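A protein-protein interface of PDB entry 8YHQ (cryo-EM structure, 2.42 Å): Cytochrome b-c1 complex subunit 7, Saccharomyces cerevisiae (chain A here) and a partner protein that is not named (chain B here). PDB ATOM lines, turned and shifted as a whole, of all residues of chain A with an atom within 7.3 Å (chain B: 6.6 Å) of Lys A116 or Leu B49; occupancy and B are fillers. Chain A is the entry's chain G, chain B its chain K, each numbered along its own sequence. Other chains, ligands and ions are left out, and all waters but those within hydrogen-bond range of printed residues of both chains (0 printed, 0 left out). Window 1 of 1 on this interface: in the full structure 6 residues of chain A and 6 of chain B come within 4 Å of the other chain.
The side-chain amide oxygen (OD1) of Asn B42 is in hydrogen-bond range of the side-chain hydroxyl (OG) of Ser B47, 3.2 Å away.
The side-chain hydroxyl (OG) of Ser B47 sits at hydrogen-bond distance from the backbone NH (N) of Leu B49, at 3.2 Å.
The side-chain amino group (NZ) of Lys A116 is in salt-bridge range of the side-chain carboxylate (OD2) of Asp A120, at 3.3 Å.
NH2 of Arg B53 is in salt-bridge range of OD1 of Asp A120 (3.3 Å).
Hydrophobic or aromatic side chains of chain A that line the printed part of chain B: Leu A119.
Among the printed residues, 5 pairs touch across the chains.
Among the printed residues, Asp or Glu carboxylates within 4 Å of a Lys or Arg side-chain nitrogen of the other chain: Asp A120 with Arg B53 (3.3 Å).
OE1 of Glu A115 touches CB of Ser B47, at 3.9 Å.
CA of Lys A116 touches CD2 of Leu B49, 3.96 Å away.
CD2 of Leu B49 touches CD1 of Leu A119, at 3.99 Å.
Leu A119 touches Arg B53 (CB to NH2, 3.7 Å).
Lys A116 touches just one residue of chain B: Leu B49.
Printed residues of chain A within 4 Å of Leu B49: Lys A116 and Leu A119.
Printed residues of chain B within 4 Å of Asp A120: Arg B53 (3.3 Å).
Of the printed residues of chain A, Arg B53 touches Leu A119 (3.7 Å) and Asp A120 (3.3 Å).
Of the printed residues of chain A, Ser B47 touches Glu A115 (3.9 Å).
The nearest residue of chain B that does not touch Lys A116 is Arg B53 (4.9 Å).
The nearest printed residue of chain A that does not touch Ser B47 is Ala A112 (6.8 Å).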
ATOM      1  N   GLU A 110      -3.273  26.317  19.417  1.00  0.00           N
ATOM      2  CA  GLU A 110      -3.892  27.629  19.593  1.00  0.00           C
ATOM      3  C   GLU A 110      -4.295  28.237  18.255  1.00  0.00           C
ATOM      4  O   GLU A 110      -5.371  28.833  18.140  1.00  0.00           O
ATOM      5  CB  GLU A 110      -2.944  28.575  20.335  1.00  0.00           C
ATOM      6  CG  GLU A 110      -3.150  28.628  21.829  1.00  0.00           C
ATOM      7  CD  GLU A 110      -2.147  29.511  22.533  1.00  0.00           C
ATOM      8  OE1 GLU A 110      -1.316  30.137  21.845  1.00  0.00           O
ATOM      9  OE2 GLU A 110      -2.188  29.576  23.781  1.00  0.00           O
ATOM     10  N   ALA A 111      -3.441  28.109  17.241  1.00  0.00           N
ATOM     11  CA  ALA A 111      -3.731  28.692  15.936  1.00  0.00           C
ATOM     12  C   ALA A 111      -4.935  28.033  15.278  1.00  0.00           C
ATOM     13  O   ALA A 111      -5.645  28.668  14.491  1.00  0.00           O
ATOM     14  CB  ALA A 111      -2.505  28.581  15.035  1.00  0.00           C
ATOM     15  N   ALA A 112      -5.176  26.758  15.575  1.00  0.00           N
ATOM     16  CA  ALA A 112      -6.318  26.060  15.003  1.00  0.00           C
ATOM     17  C   ALA A 112      -7.615  26.448  15.697  1.00  0.00           C
ATOM     18  O   ALA A 112      -8.678  26.462  15.069  1.00  0.00           O
ATOM     19  CB  ALA A 112      -6.100  24.552  15.083  1.00  0.00           C
ATOM     20  N   ALA A 113      -7.551  26.753  16.993  1.00  0.00           N
ATOM     21  CA  ALA A 113      -8.744  27.164  17.720  1.00  0.00           C
ATOM     22  C   ALA A 113      -9.189  28.565  17.323  1.00  0.00           C
ATOM     23  O   ALA A 113     -10.385  28.867  17.356  1.00  0.00           O
ATOM     24  CB  ALA A 113      -8.486  27.083  19.220  1.00  0.00           C
ATOM     25  N   LYS A 114      -8.247  29.426  16.945  1.00  0.00           N
ATOM     26  CA  LYS A 114      -8.594  30.764  16.483  1.00  0.00           C
ATOM     27  C   LYS A 114      -9.183  30.732  15.077  1.00  0.00           C
ATOM     28  O   LYS A 114     -10.136  31.461  14.783  1.00  0.00           O
ATOM     29  CB  LYS A 114      -7.357  31.659  16.537  1.00  0.00           C
ATOM     30  CG  LYS A 114      -7.609  33.115  16.256  1.00  0.00           C
ATOM     31  CD  LYS A 114      -6.321  33.894  16.265  1.00  0.00           C
ATOM     32  CE  LYS A 114      -6.553  35.354  15.986  1.00  0.00           C
ATOM     33  NZ  LYS A 114      -6.964  35.580  14.585  1.00  0.00           N
ATOM     34  N   GLU A 115      -8.624  29.905  14.193  1.00  0.00           N
ATOM     35  CA  GLU A 115      -9.170  29.761  12.848  1.00  0.00           C
ATOM     36  C   GLU A 115     -10.580  29.184  12.874  1.00  0.00           C
ATOM     37  O   GLU A 115     -11.463  29.669  12.160  1.00  0.00           O
ATOM     38  CB  GLU A 115      -8.239  28.888  12.008  1.00  0.00           C
ATOM     39  CG  GLU A 115      -8.532  28.869  10.522  1.00  0.00           C
ATOM     40  CD  GLU A 115      -7.965  27.652   9.822  1.00  0.00           C
ATOM     41  OE1 GLU A 115      -8.155  26.522  10.325  1.00  0.00           O
ATOM     42  OE2 GLU A 115      -7.327  27.824   8.765  1.00  0.00           O
ATOM     43  N   LYS A 116     -10.808  28.142  13.675  1.00  0.00           N
ATOM     44  CA  LYS A 116     -12.145  27.569  13.795  1.00  0.00           C
ATOM     45  C   LYS A 116     -13.142  28.597  14.286  1.00  0.00           C
ATOM     46  O   LYS A 116     -14.296  28.613  13.849  1.00  0.00           O
ATOM     47  CB  LYS A 116     -12.136  26.384  14.763  1.00  0.00           C
ATOM     48  CG  LYS A 116     -13.455  25.654  14.886  1.00  0.00           C
ATOM     49  CD  LYS A 116     -13.393  24.563  15.913  1.00  0.00           C
ATOM     50  CE  LYS A 116     -14.625  23.681  15.884  1.00  0.00           C
ATOM     51  NZ  LYS A 116     -15.895  24.435  15.760  1.00  0.00           N
ATOM     52  N   ASP A 117     -12.830  29.396  15.290  1.00  0.00           N
ATOM     53  CA  ASP A 117     -13.676  30.422  15.948  1.00  0.00           C
ATOM     54  C   ASP A 117     -13.954  31.627  15.062  1.00  0.00           C
ATOM     55  O   ASP A 117     -15.068  32.124  15.056  1.00  0.00           O
ATOM     56  CB  ASP A 117     -13.033  31.084  17.144  1.00  0.00           C
ATOM     57  CG  ASP A 117     -13.960  31.401  18.288  1.00  0.00           C
ATOM     58  OD1 ASP A 117     -15.145  31.042  18.214  1.00  0.00           O
ATOM     59  OD2 ASP A 117     -13.470  31.962  19.260  1.00  0.00           O
ATOM     60  N   GLU A 118     -12.999  32.057  14.333  1.00  0.00           N
ATOM     61  CA  GLU A 118     -13.329  33.094  13.365  1.00  0.00           C
ATOM     62  C   GLU A 118     -14.341  32.611  12.336  1.00  0.00           C
ATOM     63  O   GLU A 118     -15.207  33.384  11.918  1.00  0.00           O
ATOM     64  CB  GLU A 118     -12.076  33.576  12.639  1.00  0.00           C
ATOM     65  CG  GLU A 118     -11.082  34.311  13.499  1.00  0.00           C
ATOM     66  CD  GLU A 118      -9.740  34.476  12.819  1.00  0.00           C
ATOM     67  OE1 GLU A 118      -9.177  33.464  12.350  1.00  0.00           O
ATOM     68  OE2 GLU A 118      -9.244  35.620  12.751  1.00  0.00           O
ATOM     69  N   LEU A 119     -14.244  31.351  11.909  1.00  0.00           N
ATOM     70  CA  LEU A 119     -15.125  30.827  10.874  1.00  0.00           C
ATOM     71  C   LEU A 119     -16.554  30.627  11.355  1.00  0.00           C
ATOM     72  O   LEU A 119     -17.462  30.526  10.527  1.00  0.00           O
ATOM     73  CB  LEU A 119     -14.584  29.502  10.337  1.00  0.00           C
ATOM     74  CG  LEU A 119     -13.323  29.552   9.472  1.00  0.00           C
ATOM     75  CD1 LEU A 119     -12.814  28.151   9.236  1.00  0.00           C
ATOM     76  CD2 LEU A 119     -13.573  30.246   8.160  1.00  0.00           C
ATOM     77  N   ASP A 120     -16.771  30.568  12.663  1.00  0.00           N
ATOM     78  CA  ASP A 120     -18.092  30.371  13.235  1.00  0.00           C
ATOM     79  C   ASP A 120     -18.843  31.673  13.488  1.00  0.00           C
ATOM     80  O   ASP A 120     -19.985  31.623  13.953  1.00  0.00           O
ATOM     81  CB  ASP A 120     -17.979  29.589  14.543  1.00  0.00           C
ATOM     82  CG  ASP A 120     -17.471  28.177  14.342  1.00  0.00           C
ATOM     83  OD1 ASP A 120     -17.437  27.710  13.186  1.00  0.00           O
ATOM     84  OD2 ASP A 120     -17.118  27.525  15.345  1.00  0.00           O
ATOM     85  N   ASN A 121     -18.234  32.825  13.217  1.00  0.00           N
ATOM     86  CA  ASN A 121     -18.853  34.128  13.448  1.00  0.00           C
ATOM     87  C   ASN A 121     -18.535  35.089  12.302  1.00  0.00           C
ATOM     88  O   ASN A 121     -18.284  36.276  12.509  1.00  0.00           O
ATOM     89  CB  ASN A 121     -18.363  34.711  14.769  1.00  0.00           C
ATOM     90  CG  ASN A 121     -18.681  33.816  15.953  1.00  0.00           C
ATOM     91  OD1 ASN A 121     -17.795  33.438  16.717  1.00  0.00           O
ATOM     92  ND2 ASN A 121     -19.945  33.464  16.104  1.00  0.00           N
ATOM     93  N   ASN B  42      -4.670  18.512   5.684  1.00  0.00           N
ATOM     94  CA  ASN B  42      -4.005  19.805   5.681  1.00  0.00           C
ATOM     95  C   ASN B  42      -2.925  19.881   4.615  1.00  0.00           C
ATOM     96  O   ASN B  42      -2.186  18.923   4.374  1.00  0.00           O
ATOM     97  CB  ASN B  42      -3.391  20.091   7.043  1.00  0.00           C
ATOM     98  CG  ASN B  42      -4.418  20.255   8.126  1.00  0.00           C
ATOM     99  OD1 ASN B  42      -5.617  20.298   7.873  1.00  0.00           O
ATOM    100  ND2 ASN B  42      -3.949  20.352   9.350  1.00  0.00           N
ATOM    101  N   ARG B  46      -2.868  25.791   3.339  1.00  0.00           N
ATOM    102  CA  ARG B  46      -4.185  25.933   3.939  1.00  0.00           C
ATOM    103  C   ARG B  46      -4.583  24.643   4.640  1.00  0.00           C
ATOM    104  O   ARG B  46      -4.079  23.563   4.330  1.00  0.00           O
ATOM    105  CB  ARG B  46      -5.234  26.368   2.894  1.00  0.00           C
ATOM    106  CG  ARG B  46      -5.907  25.306   2.014  1.00  0.00           C
ATOM    107  CD  ARG B  46      -7.305  25.713   1.590  1.00  0.00           C
ATOM    108  NE  ARG B  46      -7.301  26.641   0.466  1.00  0.00           N
ATOM    109  CZ  ARG B  46      -7.102  26.299  -0.804  1.00  0.00           C
ATOM    110  NH1 ARG B  46      -7.134  27.232  -1.736  1.00  0.00           N
ATOM    111  NH2 ARG B  46      -6.863  25.044  -1.156  1.00  0.00           N
ATOM    112  N   SER B  47      -5.513  24.776   5.578  1.00  0.00           N
ATOM    113  CA  SER B  47      -5.963  23.665   6.392  1.00  0.00           C
ATOM    114  C   SER B  47      -7.105  22.911   5.717  1.00  0.00           C
ATOM    115  O   SER B  47      -7.714  23.373   4.750  1.00  0.00           O
ATOM    116  CB  SER B  47      -6.405  24.160   7.763  1.00  0.00           C
ATOM    117  OG  SER B  47      -7.058  23.140   8.481  1.00  0.00           O
ATOM    118  N   ALA B  48      -7.392  21.725   6.253  1.00  0.00           N
ATOM    119  CA  ALA B  48      -8.510  20.924   5.778  1.00  0.00           C
ATOM    120  C   ALA B  48      -9.853  21.519   6.164  1.00  0.00           C
ATOM    121  O   ALA B  48     -10.855  21.230   5.503  1.00  0.00           O
ATOM    122  CB  ALA B  48      -8.413  19.502   6.323  1.00  0.00           C
ATOM    123  N   LEU B  49      -9.900  22.330   7.218  1.00  0.00           N
ATOM    124  CA  LEU B  49     -11.144  22.966   7.623  1.00  0.00           C
ATOM    125  C   LEU B  49     -11.507  24.107   6.683  1.00  0.00           C
ATOM    126  O   LEU B  49     -12.661  24.225   6.265  1.00  0.00           O
ATOM    127  CB  LEU B  49     -11.021  23.463   9.061  1.00  0.00           C
ATOM    128  CG  LEU B  49     -12.195  24.189   9.714  1.00  0.00           C
ATOM    129  CD1 LEU B  49     -13.364  23.283   9.898  1.00  0.00           C
ATOM    130  CD2 LEU B  49     -11.783  24.746  11.038  1.00  0.00           C
ATOM    131  N   LYS B  50     -10.533  24.938   6.325  1.00  0.00           N
ATOM    132  CA  LYS B  50     -10.800  26.074   5.456  1.00  0.00           C
ATOM    133  C   LYS B  50     -11.209  25.643   4.054  1.00  0.00           C
ATOM    134  O   LYS B  50     -11.999  26.335   3.405  1.00  0.00           O
ATOM    135  CB  LYS B  50      -9.576  26.976   5.394  1.00  0.00           C
ATOM    136  CG  LYS B  50      -9.907  28.417   5.152  1.00  0.00           C
ATOM    137  CD  LYS B  50      -8.759  29.135   4.498  1.00  0.00           C
ATOM    138  CE  LYS B  50      -8.899  30.653   4.585  1.00  0.00           C
ATOM    139  NZ  LYS B  50      -7.573  31.338   4.563  1.00  0.00           N
ATOM    140  N   LEU B  51     -10.678  24.524   3.565  1.00  0.00           N
ATOM    141  CA  LEU B  51     -11.074  24.021   2.254  1.00  0.00           C
ATOM    142  C   LEU B  51     -12.545  23.628   2.235  1.00  0.00           C
ATOM    143  O   LEU B  51     -13.264  23.912   1.271  1.00  0.00           O
ATOM    144  CB  LEU B  51     -10.193  22.835   1.874  1.00  0.00           C
ATOM    145  CG  LEU B  51     -10.358  22.231   0.480  1.00  0.00           C
ATOM    146  CD1 LEU B  51      -9.728  23.114  -0.563  1.00  0.00           C
ATOM    147  CD2 LEU B  51      -9.763  20.856   0.446  1.00  0.00           C
ATOM    148  N   VAL B  52     -13.009  22.964   3.290  1.00  0.00           N
ATOM    149  CA  VAL B  52     -14.407  22.554   3.366  1.00  0.00           C
ATOM    150  C   VAL B  52     -15.317  23.775   3.450  1.00  0.00           C
ATOM    151  O   VAL B  52     -16.393  23.810   2.846  1.00  0.00           O
ATOM    152  CB  VAL B  52     -14.620  21.600   4.556  1.00  0.00           C
ATOM    153  CG1 VAL B  52     -16.083  21.441   4.890  1.00  0.00           C
ATOM    154  CG2 VAL B  52     -14.016  20.259   4.263  1.00  0.00           C
ATOM    155  N   ARG B  53     -14.898  24.796   4.199  1.00  0.00           N
ATOM    156  CA  ARG B  53     -15.750  25.962   4.404  1.00  0.00           C
ATOM    157  C   ARG B  53     -15.775  26.860   3.173  1.00  0.00           C
ATOM    158  O   ARG B  53     -16.828  27.395   2.814  1.00  0.00           O
ATOM    159  CB  ARG B  53     -15.284  26.748   5.628  1.00  0.00           C
ATOM    160  CG  ARG B  53     -15.296  25.983   6.937  1.00  0.00           C
ATOM    161  CD  ARG B  53     -16.663  25.615   7.397  1.00  0.00           C
ATOM    162  NE  ARG B  53     -16.639  24.955   8.698  1.00  0.00           N
ATOM    163  CZ  ARG B  53     -16.825  25.544   9.876  1.00  0.00           C
ATOM    164  NH1 ARG B  53     -16.777  24.814  10.972  1.00  0.00           N
ATOM    165  NH2 ARG B  53     -17.060  26.839   9.987  1.00  0.00           N
ATOM    166  N   GLU B  54     -14.629  27.042   2.519  1.00  0.00           N
ATOM    167  CA  GLU B  54     -14.569  27.888   1.333  1.00  0.00           C
ATOM    168  C   GLU B  54     -15.365  27.293   0.179  1.00  0.00           C
ATOM    169  O   GLU B  54     -16.105  28.005  -0.508  1.00  0.00           O
ATOM    170  CB  GLU B  54     -13.120  28.097   0.916  1.00  0.00           C
ATOM    171  CG  GLU B  54     -12.365  29.085   1.736  1.00  0.00           C
ATOM    172  CD  GLU B  54     -11.002  29.380   1.151  1.00  0.00           C
ATOM    173  OE1 GLU B  54     -10.552  28.608   0.280  1.00  0.00           O
ATOM    174  OE2 GLU B  54     -10.381  30.381   1.560  1.00  0.00           O
